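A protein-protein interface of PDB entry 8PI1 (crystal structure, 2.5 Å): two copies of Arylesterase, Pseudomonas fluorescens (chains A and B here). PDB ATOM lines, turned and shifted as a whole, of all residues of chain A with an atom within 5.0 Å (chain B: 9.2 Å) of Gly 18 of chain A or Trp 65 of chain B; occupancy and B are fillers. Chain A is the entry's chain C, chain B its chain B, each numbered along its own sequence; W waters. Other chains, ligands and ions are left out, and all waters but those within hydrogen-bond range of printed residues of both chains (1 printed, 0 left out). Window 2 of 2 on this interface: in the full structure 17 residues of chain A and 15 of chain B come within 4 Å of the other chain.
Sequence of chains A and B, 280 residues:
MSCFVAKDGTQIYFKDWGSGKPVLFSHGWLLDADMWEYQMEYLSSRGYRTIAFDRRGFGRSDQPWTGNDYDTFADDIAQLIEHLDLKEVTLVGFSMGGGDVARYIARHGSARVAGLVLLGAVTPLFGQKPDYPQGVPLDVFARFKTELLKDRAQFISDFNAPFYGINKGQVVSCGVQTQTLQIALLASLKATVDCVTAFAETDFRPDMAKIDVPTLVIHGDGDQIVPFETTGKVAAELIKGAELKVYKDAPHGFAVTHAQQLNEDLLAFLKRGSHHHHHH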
ATOM      1  N   ASP A  16     -17.097  11.682  24.324  1.00  0.00           N
ATOM      2  CA  ASP A  16     -18.310  11.638  23.524  1.00  0.00           C
ATOM      3  C   ASP A  16     -18.312  12.843  22.581  1.00  0.00           C
ATOM      4  O   ASP A  16     -18.590  13.964  23.004  1.00  0.00           O
ATOM      5  CB  ASP A  16     -19.538  11.542  24.432  1.00  0.00           C
ATOM      6  CG  ASP A  16     -20.857  11.305  23.714  1.00  0.00           C
ATOM      7  OD1 ASP A  16     -20.848  11.158  22.473  1.00  0.00           O
ATOM      8  OD2 ASP A  16     -21.895  11.272  24.405  1.00  0.00           O
ATOM      9  N   TRP A  17     -17.974  12.599  21.305  1.00  0.00           N
ATOM     10  CA  TRP A  17     -17.836  13.660  20.316  1.00  0.00           C
ATOM     11  C   TRP A  17     -18.960  13.593  19.287  1.00  0.00           C
ATOM     12  O   TRP A  17     -19.307  12.512  18.810  1.00  0.00           O
ATOM     13  CB  TRP A  17     -16.472  13.591  19.612  1.00  0.00           C
ATOM     14  CG  TRP A  17     -15.295  14.018  20.432  1.00  0.00           C
ATOM     15  CD1 TRP A  17     -15.303  14.492  21.713  1.00  0.00           C
ATOM     16  CD2 TRP A  17     -13.914  14.000  20.021  1.00  0.00           C
ATOM     17  NE1 TRP A  17     -14.028  14.771  22.124  1.00  0.00           N
ATOM     18  CE2 TRP A  17     -13.153  14.477  21.112  1.00  0.00           C
ATOM     19  CE3 TRP A  17     -13.246  13.621  18.849  1.00  0.00           C
ATOM     20  CZ2 TRP A  17     -11.765  14.592  21.056  1.00  0.00           C
ATOM     21  CZ3 TRP A  17     -11.873  13.732  18.796  1.00  0.00           C
ATOM     22  CH2 TRP A  17     -11.145  14.215  19.886  1.00  0.00           C
ATOM     23  N   GLY A  18     -19.489  14.772  18.933  1.00  0.00           N
ATOM     24  CA  GLY A  18     -20.391  14.937  17.803  1.00  0.00           C
ATOM     25  C   GLY A  18     -21.779  14.356  18.059  1.00  0.00           C
ATOM     26  O   GLY A  18     -22.139  14.050  19.194  1.00  0.00           O
ATOM     27  N   SER A  19     -22.547  14.217  16.974  1.00  0.00           N
ATOM     28  CA  SER A  19     -23.892  13.669  17.018  1.00  0.00           C
ATOM     29  C   SER A  19     -24.175  12.884  15.737  1.00  0.00           C
ATOM     30  O   SER A  19     -23.471  13.038  14.741  1.00  0.00           O
ATOM     31  CB  SER A  19     -24.898  14.762  17.233  1.00  0.00           C
ATOM     32  OG  SER A  19     -24.802  15.725  16.198  1.00  0.00           O
ATOM     33  N   GLY A  20     -25.215  12.043  15.783  1.00  0.00           N
ATOM     34  CA  GLY A  20     -25.567  11.164  14.680  1.00  0.00           C
ATOM     35  C   GLY A  20     -25.464   9.698  15.091  1.00  0.00           C
ATOM     36  O   GLY A  20     -25.565   9.381  16.276  1.00  0.00           O
ATOM     37  N   MET A  40     -11.740   9.533  15.083  1.00  0.00           N
ATOM     38  CA  MET A  40     -12.868  10.175  15.738  1.00  0.00           C
ATOM     39  C   MET A  40     -13.122  11.546  15.117  1.00  0.00           C
ATOM     40  O   MET A  40     -14.259  11.865  14.779  1.00  0.00           O
ATOM     41  CB  MET A  40     -12.617  10.319  17.241  1.00  0.00           C
ATOM     42  CG  MET A  40     -12.874   9.037  18.013  1.00  0.00           C
ATOM     43  SD  MET A  40     -12.535   9.218  19.787  1.00  0.00           S
ATOM     44  CE  MET A  40     -14.091   9.908  20.350  1.00  0.00           C
ATOM     45  N   GLU A  41     -12.058  12.344  14.948  1.00  0.00           N
ATOM     46  CA  GLU A  41     -12.206  13.664  14.352  1.00  0.00           C
ATOM     47  C   GLU A  41     -12.705  13.519  12.916  1.00  0.00           C
ATOM     48  O   GLU A  41     -13.548  14.296  12.476  1.00  0.00           O
ATOM     49  CB  GLU A  41     -10.907  14.470  14.428  1.00  0.00           C
ATOM     50  CG  GLU A  41     -11.063  15.920  13.990  1.00  0.00           C
ATOM     51  CD  GLU A  41     -11.127  16.189  12.494  1.00  0.00           C
ATOM     52  OE1 GLU A  41     -10.629  15.352  11.710  1.00  0.00           O
ATOM     53  OE2 GLU A  41     -11.701  17.228  12.108  1.00  0.00           O
ATOM     54  N   SER A  44     -16.537  12.345  13.063  1.00  0.00           N
ATOM     55  CA  SER A  44     -17.395  13.296  13.756  1.00  0.00           C
ATOM     56  C   SER A  44     -17.513  14.616  12.996  1.00  0.00           C
ATOM     57  O   SER A  44     -18.541  15.282  13.078  1.00  0.00           O
ATOM     58  CB  SER A  44     -16.975  13.504  15.186  1.00  0.00           C
ATOM     59  OG  SER A  44     -17.404  12.423  16.000  1.00  0.00           O
ATOM     60  N   SER A  45     -16.467  14.986  12.253  1.00  0.00           N
ATOM     61  CA  SER A  45     -16.546  16.169  11.412  1.00  0.00           C
ATOM     62  C   SER A  45     -17.237  15.826  10.090  1.00  0.00           C
ATOM     63  O   SER A  45     -17.280  16.645   9.174  1.00  0.00           O
ATOM     64  CB  SER A  45     -15.188  16.790  11.202  1.00  0.00           C
ATOM     65  OG  SER A  45     -14.351  15.924  10.453  1.00  0.00           O
ATOM     66  N   TYR A  48     -20.951  12.045  12.191  1.00  0.00           N
ATOM     67  CA  TYR A  48     -21.111  10.863  13.023  1.00  0.00           C
ATOM     68  C   TYR A  48     -20.833  11.211  14.483  1.00  0.00           C
ATOM     69  O   TYR A  48     -20.211  12.229  14.776  1.00  0.00           O
ATOM     70  CB  TYR A  48     -20.259   9.695  12.516  1.00  0.00           C
ATOM     71  CG  TYR A  48     -20.716   9.129  11.194  1.00  0.00           C
ATOM     72  CD1 TYR A  48     -20.295   9.680   9.995  1.00  0.00           C
ATOM     73  CD2 TYR A  48     -21.617   8.075  11.141  1.00  0.00           C
ATOM     74  CE1 TYR A  48     -20.727   9.180   8.777  1.00  0.00           C
ATOM     75  CE2 TYR A  48     -22.063   7.564   9.931  1.00  0.00           C
ATOM     76  CZ  TYR A  48     -21.617   8.120   8.743  1.00  0.00           C
ATOM     77  OH  TYR A  48     -22.050   7.632   7.531  1.00  0.00           O
ATOM     78  N   ARG A  49     -21.325  10.366  15.393  1.00  0.00           N
ATOM     79  CA  ARG A  49     -21.010  10.488  16.805  1.00  0.00           C
ATOM     80  C   ARG A  49     -19.976   9.423  17.161  1.00  0.00           C
ATOM     81  O   ARG A  49     -20.201   8.243  16.904  1.00  0.00           O
ATOM     82  CB  ARG A  49     -22.278  10.329  17.648  1.00  0.00           C
ATOM     83  CG  ARG A  49     -22.062  10.499  19.145  1.00  0.00           C
ATOM     84  CD  ARG A  49     -23.377  10.322  19.873  1.00  0.00           C
ATOM     85  NE  ARG A  49     -23.264  10.396  21.322  1.00  0.00           N
ATOM     86  CZ  ARG A  49     -24.277  10.226  22.164  1.00  0.00           C
ATOM     87  NH1 ARG A  49     -25.479   9.936  21.701  1.00  0.00           N
ATOM     88  NH2 ARG A  49     -24.082  10.338  23.466  1.00  0.00           N
ATOM     89  N   ASP B   8     -22.250  23.908  29.622  1.00  0.00           N
ATOM     90  CA  ASP B   8     -22.561  22.763  28.778  1.00  0.00           C
ATOM     91  C   ASP B   8     -22.191  21.460  29.482  1.00  0.00           C
ATOM     92  O   ASP B   8     -22.341  20.385  28.911  1.00  0.00           O
ATOM     93  CB  ASP B   8     -21.898  22.871  27.401  1.00  0.00           C
ATOM     94  CG  ASP B   8     -20.383  22.742  27.424  1.00  0.00           C
ATOM     95  OD1 ASP B   8     -19.814  22.637  28.530  1.00  0.00           O
ATOM     96  OD2 ASP B   8     -19.778  22.744  26.332  1.00  0.00           O
ATOM     97  N   THR B  10     -19.052  20.827  30.716  1.00  0.00           N
ATOM     98  CA  THR B  10     -17.619  20.597  30.631  1.00  0.00           C
ATOM     99  C   THR B  10     -16.970  20.923  31.975  1.00  0.00           C
ATOM    100  O   THR B  10     -17.205  21.986  32.546  1.00  0.00           O
ATOM    101  CB  THR B  10     -16.983  21.420  29.504  1.00  0.00           C
ATOM    102  OG1 THR B  10     -17.558  21.006  28.265  1.00  0.00           O
ATOM    103  CG2 THR B  10     -15.483  21.253  29.425  1.00  0.00           C
ATOM    104  N   ARG B  56     -10.754  24.405  27.992  1.00  0.00           N
ATOM    105  CA  ARG B  56     -11.468  23.217  27.543  1.00  0.00           C
ATOM    106  C   ARG B  56     -10.716  22.582  26.374  1.00  0.00           C
ATOM    107  O   ARG B  56     -10.338  23.264  25.424  1.00  0.00           O
ATOM    108  CB  ARG B  56     -12.928  23.539  27.207  1.00  0.00           C
ATOM    109  CG  ARG B  56     -13.122  24.621  26.151  1.00  0.00           C
ATOM    110  CD  ARG B  56     -14.538  24.724  25.604  1.00  0.00           C
ATOM    111  NE  ARG B  56     -15.548  25.110  26.582  1.00  0.00           N
ATOM    112  CZ  ARG B  56     -16.761  24.574  26.686  1.00  0.00           C
ATOM    113  NH1 ARG B  56     -17.178  23.666  25.818  1.00  0.00           N
ATOM    114  NH2 ARG B  56     -17.569  24.969  27.653  1.00  0.00           N
ATOM    115  N   GLY B  57     -10.484  21.268  26.479  1.00  0.00           N
ATOM    116  CA  GLY B  57      -9.753  20.519  25.470  1.00  0.00           C
ATOM    117  C   GLY B  57      -8.245  20.514  25.721  1.00  0.00           C
ATOM    118  O   GLY B  57      -7.483  20.017  24.896  1.00  0.00           O
ATOM    119  N   ASP B  62     -11.816  18.566  30.625  1.00  0.00           N
ATOM    120  CA  ASP B  62     -12.577  17.747  29.693  1.00  0.00           C
ATOM    121  C   ASP B  62     -12.321  18.206  28.258  1.00  0.00           C
ATOM    122  O   ASP B  62     -11.879  19.330  28.024  1.00  0.00           O
ATOM    123  CB  ASP B  62     -14.073  17.801  30.015  1.00  0.00           C
ATOM    124  CG  ASP B  62     -14.478  16.958  31.212  1.00  0.00           C
ATOM    125  OD1 ASP B  62     -13.632  16.175  31.691  1.00  0.00           O
ATOM    126  OD2 ASP B  62     -15.643  17.087  31.650  1.00  0.00           O
ATOM    127  N   GLN B  63     -12.632  17.326  27.299  1.00  0.00           N
ATOM    128  CA  GLN B  63     -12.349  17.569  25.892  1.00  0.00           C
ATOM    129  C   GLN B  63     -13.641  17.511  25.081  1.00  0.00           C
ATOM    130  O   GLN B  63     -13.879  16.532  24.376  1.00  0.00           O
ATOM    131  CB  GLN B  63     -11.377  16.510  25.372  1.00  0.00           C
ATOM    132  CG  GLN B  63     -10.046  16.485  26.106  1.00  0.00           C
ATOM    133  CD  GLN B  63      -9.105  15.461  25.521  1.00  0.00           C
ATOM    134  OE1 GLN B  63      -9.496  14.622  24.711  1.00  0.00           O
ATOM    135  NE2 GLN B  63      -7.850  15.525  25.933  1.00  0.00           N
ATOM    136  N   PRO B  64     -14.505  18.555  25.134  1.00  0.00           N
ATOM    137  CA  PRO B  64     -15.774  18.539  24.405  1.00  0.00           C
ATOM    138  C   PRO B  64     -15.576  18.809  22.915  1.00  0.00           C
ATOM    139  O   PRO B  64     -14.628  19.481  22.514  1.00  0.00           O
ATOM    140  CB  PRO B  64     -16.556  19.685  25.060  1.00  0.00           C
ATOM    141  CG  PRO B  64     -15.484  20.671  25.484  1.00  0.00           C
ATOM    142  CD  PRO B  64     -14.298  19.813  25.873  1.00  0.00           C
ATOM    143  N   TRP B  65     -16.490  18.274  22.102  1.00  0.00           N
ATOM    144  CA  TRP B  65     -16.455  18.457  20.663  1.00  0.00           C
ATOM    145  C   TRP B  65     -16.861  19.885  20.306  1.00  0.00           C
ATOM    146  O   TRP B  65     -16.273  20.484  19.412  1.00  0.00           O
ATOM    147  CB  TRP B  65     -17.345  17.414  19.977  1.00  0.00           C
ATOM    148  CG  TRP B  65     -17.395  17.518  18.485  1.00  0.00           C
ATOM    149  CD1 TRP B  65     -18.401  18.057  17.737  1.00  0.00           C
ATOM    150  CD2 TRP B  65     -16.416  17.035  17.548  1.00  0.00           C
ATOM    151  NE1 TRP B  65     -18.107  17.964  16.403  1.00  0.00           N
ATOM    152  CE2 TRP B  65     -16.899  17.339  16.254  1.00  0.00           C
ATOM    153  CE3 TRP B  65     -15.179  16.388  17.669  1.00  0.00           C
ATOM    154  CZ2 TRP B  65     -16.185  17.020  15.100  1.00  0.00           C
ATOM    155  CZ3 TRP B  65     -14.476  16.071  16.527  1.00  0.00           C
ATOM    156  CH2 TRP B  65     -14.973  16.387  15.262  1.00  0.00           C
ATOM    157  N   THR B  66     -17.851  20.434  21.021  1.00  0.00           N
ATOM    158  CA  THR B  66     -18.410  21.735  20.683  1.00  0.00           C
ATOM    159  C   THR B  66     -17.887  22.808  21.633  1.00  0.00           C
ATOM    160  O   THR B  66     -17.415  22.501  22.727  1.00  0.00           O
ATOM    161  CB  THR B  66     -19.942  21.731  20.762  1.00  0.00           C
ATOM    162  OG1 THR B  66     -20.290  21.334  22.088  1.00  0.00           O
ATOM    163  CG2 THR B  66     -20.594  20.807  19.758  1.00  0.00           C
ATOM    164  N   GLY B  67     -17.991  24.066  21.190  1.00  0.00           N
ATOM    165  CA  GLY B  67     -17.745  25.226  22.031  1.00  0.00           C
ATOM    166  C   GLY B  67     -16.270  25.615  22.084  1.00  0.00           C
ATOM    167  O   GLY B  67     -15.837  26.255  23.040  1.00  0.00           O
ATOM    168  N   ASN B  68     -15.508  25.227  21.054  1.00  0.00           N
ATOM    169  CA  ASN B  68     -14.103  25.593  20.955  1.00  0.00           C
ATOM    170  C   ASN B  68     -13.990  26.887  20.153  1.00  0.00           C
ATOM    171  O   ASN B  68     -13.481  26.905  19.031  1.00  0.00           O
ATOM    172  CB  ASN B  68     -13.242  24.441  20.425  1.00  0.00           C
ATOM    173  CG  ASN B  68     -13.263  23.211  21.311  1.00  0.00           C
ATOM    174  OD1 ASN B  68     -13.738  22.153  20.899  1.00  0.00           O
ATOM    175  ND2 ASN B  68     -12.748  23.338  22.526  1.00  0.00           N
ATOM    176  N   ASP B  69     -14.496  27.968  20.756  1.00  0.00           N
ATOM    177  CA  ASP B  69     -14.571  29.280  20.140  1.00  0.00           C
ATOM    178  C   ASP B  69     -14.415  30.325  21.241  1.00  0.00           C
ATOM    179  O   ASP B  69     -14.594  30.014  22.417  1.00  0.00           O
ATOM    180  CB  ASP B  69     -15.890  29.445  19.382  1.00  0.00           C
ATOM    181  CG  ASP B  69     -17.102  29.267  20.280  1.00  0.00           C
ATOM    182  OD1 ASP B  69     -17.380  30.182  21.080  1.00  0.00           O
ATOM    183  OD2 ASP B  69     -17.740  28.202  20.197  1.00  0.00           O
ATOM    184  N   LEU B 149      -3.499  17.239  11.402  1.00  0.00           N
ATOM    185  CA  LEU B 149      -4.445  16.164  11.146  1.00  0.00           C
ATOM    186  C   LEU B 149      -3.741  14.946  10.550  1.00  0.00           C
ATOM    187  O   LEU B 149      -4.388  13.947  10.243  1.00  0.00           O
ATOM    188  CB  LEU B 149      -5.591  16.665  10.257  1.00  0.00           C
ATOM    189  CG  LEU B 149      -6.641  17.538  10.952  1.00  0.00           C
ATOM    190  CD1 LEU B 149      -7.794  17.851  10.012  1.00  0.00           C
ATOM    191  CD2 LEU B 149      -7.162  16.880  12.223  1.00  0.00           C
ATOM    192  N   SER B 188      -6.716  17.695  23.471  1.00  0.00           N
ATOM    193  CA  SER B 188      -7.538  17.073  22.446  1.00  0.00           C
ATOM    194  C   SER B 188      -7.037  17.477  21.062  1.00  0.00           C
ATOM    195  O   SER B 188      -6.603  18.613  20.860  1.00  0.00           O
ATOM    196  CB  SER B 188      -8.975  17.468  22.622  1.00  0.00           C
ATOM    197  OG  SER B 188      -9.708  17.228  21.431  1.00  0.00           O
ATOM    198  N   LEU B 189      -7.123  16.533  20.117  1.00  0.00           N
ATOM    199  CA  LEU B 189      -6.825  16.810  18.721  1.00  0.00           C
ATOM    200  C   LEU B 189      -7.825  17.828  18.174  1.00  0.00           C
ATOM    201  O   LEU B 189      -7.458  18.706  17.391  1.00  0.00           O
ATOM    202  CB  LEU B 189      -6.878  15.504  17.921  1.00  0.00           C
ATOM    203  CG  LEU B 189      -6.784  15.668  16.405  1.00  0.00           C
ATOM    204  CD1 LEU B 189      -5.388  16.113  15.991  1.00  0.00           C
ATOM    205  CD2 LEU B 189      -7.177  14.381  15.692  1.00  0.00           C
ATOM    206  N   LYS B 190      -9.087  17.697  18.608  1.00  0.00           N
ATOM    207  CA  LYS B 190     -10.169  18.549  18.146  1.00  0.00           C
ATOM    208  C   LYS B 190      -9.934  19.981  18.620  1.00  0.00           C
ATOM    209  O   LYS B 190      -9.958  20.915  17.819  1.00  0.00           O
ATOM    210  CB  LYS B 190     -11.525  17.981  18.581  1.00  0.00           C
ATOM    211  CG  LYS B 190     -12.741  18.848  18.274  1.00  0.00           C
ATOM    212  CD  LYS B 190     -12.876  19.247  16.818  1.00  0.00           C
ATOM    213  CE  LYS B 190     -14.227  19.848  16.500  1.00  0.00           C
ATOM    214  NZ  LYS B 190     -14.224  20.514  15.177  1.00  0.00           N
ATOM    215  N   ALA B 191      -9.687  20.137  19.924  1.00  0.00           N
ATOM    216  CA  ALA B 191      -9.472  21.445  20.517  1.00  0.00           C
ATOM    217  C   ALA B 191      -8.310  22.149  19.822  1.00  0.00           C
ATOM    218  O   ALA B 191      -8.393  23.348  19.551  1.00  0.00           O
ATOM    219  CB  ALA B 191      -9.228  21.299  21.997  1.00  0.00           C
ATOM    220  N   THR B 192      -7.247  21.382  19.525  1.00  0.00           N
ATOM    221  CA  THR B 192      -6.017  21.887  18.933  1.00  0.00           C
ATOM    222  C   THR B 192      -6.318  22.512  17.571  1.00  0.00           C
ATOM    223  O   THR B 192      -5.855  23.611  17.272  1.00  0.00           O
ATOM    224  CB  THR B 192      -4.949  20.785  18.853  1.00  0.00           C
ATOM    225  OG1 THR B 192      -4.634  20.361  20.181  1.00  0.00           O
ATOM    226  CG2 THR B 192      -3.676  21.217  18.158  1.00  0.00           C
ATOM    227  N   VAL B 193      -7.107  21.796  16.764  1.00  0.00           N
ATOM    228  CA  VAL B 193      -7.436  22.208  15.410  1.00  0.00           C
ATOM    229  C   VAL B 193      -8.430  23.366  15.467  1.00  0.00           C
ATOM    230  O   VAL B 193      -8.247  24.373  14.789  1.00  0.00           O
ATOM    231  CB  VAL B 193      -7.971  21.021  14.581  1.00  0.00           C
ATOM    232  CG1 VAL B 193      -8.614  21.468  13.276  1.00  0.00           C
ATOM    233  CG2 VAL B 193      -6.882  19.992  14.320  1.00  0.00           C
ATOM    234  N   ASP B 194      -9.470  23.213  16.294  1.00  0.00           N
ATOM    235  CA  ASP B 194     -10.504  24.223  16.437  1.00  0.00           C
ATOM    236  C   ASP B 194      -9.892  25.561  16.848  1.00  0.00           C
ATOM    237  O   ASP B 194     -10.289  26.604  16.334  1.00  0.00           O
ATOM    238  CB  ASP B 194     -11.615  23.774  17.389  1.00  0.00           C
ATOM    239  CG  ASP B 194     -12.758  23.036  16.712  1.00  0.00           C
ATOM    240  OD1 ASP B 194     -12.675  22.809  15.485  1.00  0.00           O
ATOM    241  OD2 ASP B 194     -13.739  22.708  17.415  1.00  0.00           O
ATOM    242  N   CYS B 195      -8.922  25.520  17.768  1.00  0.00           N
ATOM    243  CA  CYS B 195      -8.300  26.741  18.255  1.00  0.00           C
ATOM    244  C   CYS B 195      -7.596  27.488  17.122  1.00  0.00           C
ATOM    245  O   CYS B 195      -7.553  28.715  17.132  1.00  0.00           O
ATOM    246  CB  CYS B 195      -7.346  26.470  19.409  1.00  0.00           C
ATOM    247  SG  CYS B 195      -8.207  26.177  20.975  1.00  0.00           S
HETATM  248  O   HOH W   1     -12.739  19.509  13.038  1.00  0.00           O
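No position is printed for both chains.
CE3 of Trp 17 of chain A touches CE3 of Trp 65 of chain B, 3.6 Å away. Trp 17 of chain A touches Ser 188 of chain B (CZ2 to OG, 3.4 Å). Gly 18 of chain A touches Trp 65 of chain B. CH2 of Trp 65 of chain B touches O of Glu 41 of chain A, at 3.8 Å. OE1 of Glu 41 of chain A touches CD2 of Leu 149 of chain B, at 3.8 Å. Glu 41 of chain A touches Leu 189 of chain B (CB to CD2, 3.9 Å). Ser 44 of chain A touches Trp 65 of chain B (C to CZ2, 3.5 Å). Trp 65 of chain B touches Ser 45 of chain A.
Gly 18 of chain A touches just one residue of chain B: Trp 65 (3.5 Å). No residue of chain B comes within 4 Å of Ser 19 of chain A. Gly 20 of chain A touches none of the printed residues of chain B. Of the printed residues of chain B, Glu 41 of chain A touches Trp 65, Leu 149 and Leu 189. Ser 44 of chain A touches just one residue of chain B: Trp 65 (3.5 Å). Printed residues of chain B within 4 Å of Ser 45 of chain A: Trp 65. Of the printed residues of chain A, Gln 63 of chain B touches Trp 17. Trp 65 of chain B touches just these residues of chain A: Trp 17 (3.6 Å), Gly 18 (3.5 Å), Glu 41 (3.8 Å), Ser 44 (3.5 Å) and Ser 45 (3.5 Å). Of the printed residues of chain A, Leu 149 of chain B touches Glu 41 (3.8 Å). Printed residues of chain A within 4 Å of Ser 188 of chain B: Trp 17. The nearest residue of chain A that does not touch Trp 65 of chain B is Met 40 of chain A (4.6 Å).
O of Gln 63 of chain B is in hydrogen-bond range of NE1 of Trp 17 of chain A, 2.9 Å away.
Water W1 lies within hydrogen-bond range of OE2 of Glu 41 of chain A (2.7 Å) and NZ of Lys 190 of chain B (2.8 Å).
Printed residues of chain A that touch a printed residue of chain B: Trp 17, Gly 18, Glu 41, Ser 44 and Ser 45. Printed residues of chain B that touch a printed residue of chain A: Gln 63, Trp 65, Leu 149, Ser 188 and Leu 189. Among the printed residues, no Asp or Glu carboxylate lies within 4 Å of a Lys or Arg side-chain nitrogen of the other chain.
O of Gly 57 of chain B sits at hydrogen-bond distance from N of Ser 188 of chain B, at 2.8 Å. The side-chain amide oxygen (OD1) of Asn 68 of chain B lies close to the backbone carbonyl oxygen (O) of Trp 65 of chain B (3.4 Å). OG of Ser 188 of chain B sits at hydrogen-bond distance from N of Ala 191 of chain B. OG of Ser 44 of chain A lies within hydrogen-bond range of O of Trp 17 of chain A, at 3.4 Å. O of Glu 41 of chain A is in hydrogen-bond range of OG of Ser 45 of chain A. O of Tyr 48 of chain A sits at hydrogen-bond distance from OG of Ser 44 of chain A, at 3.1 Å.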
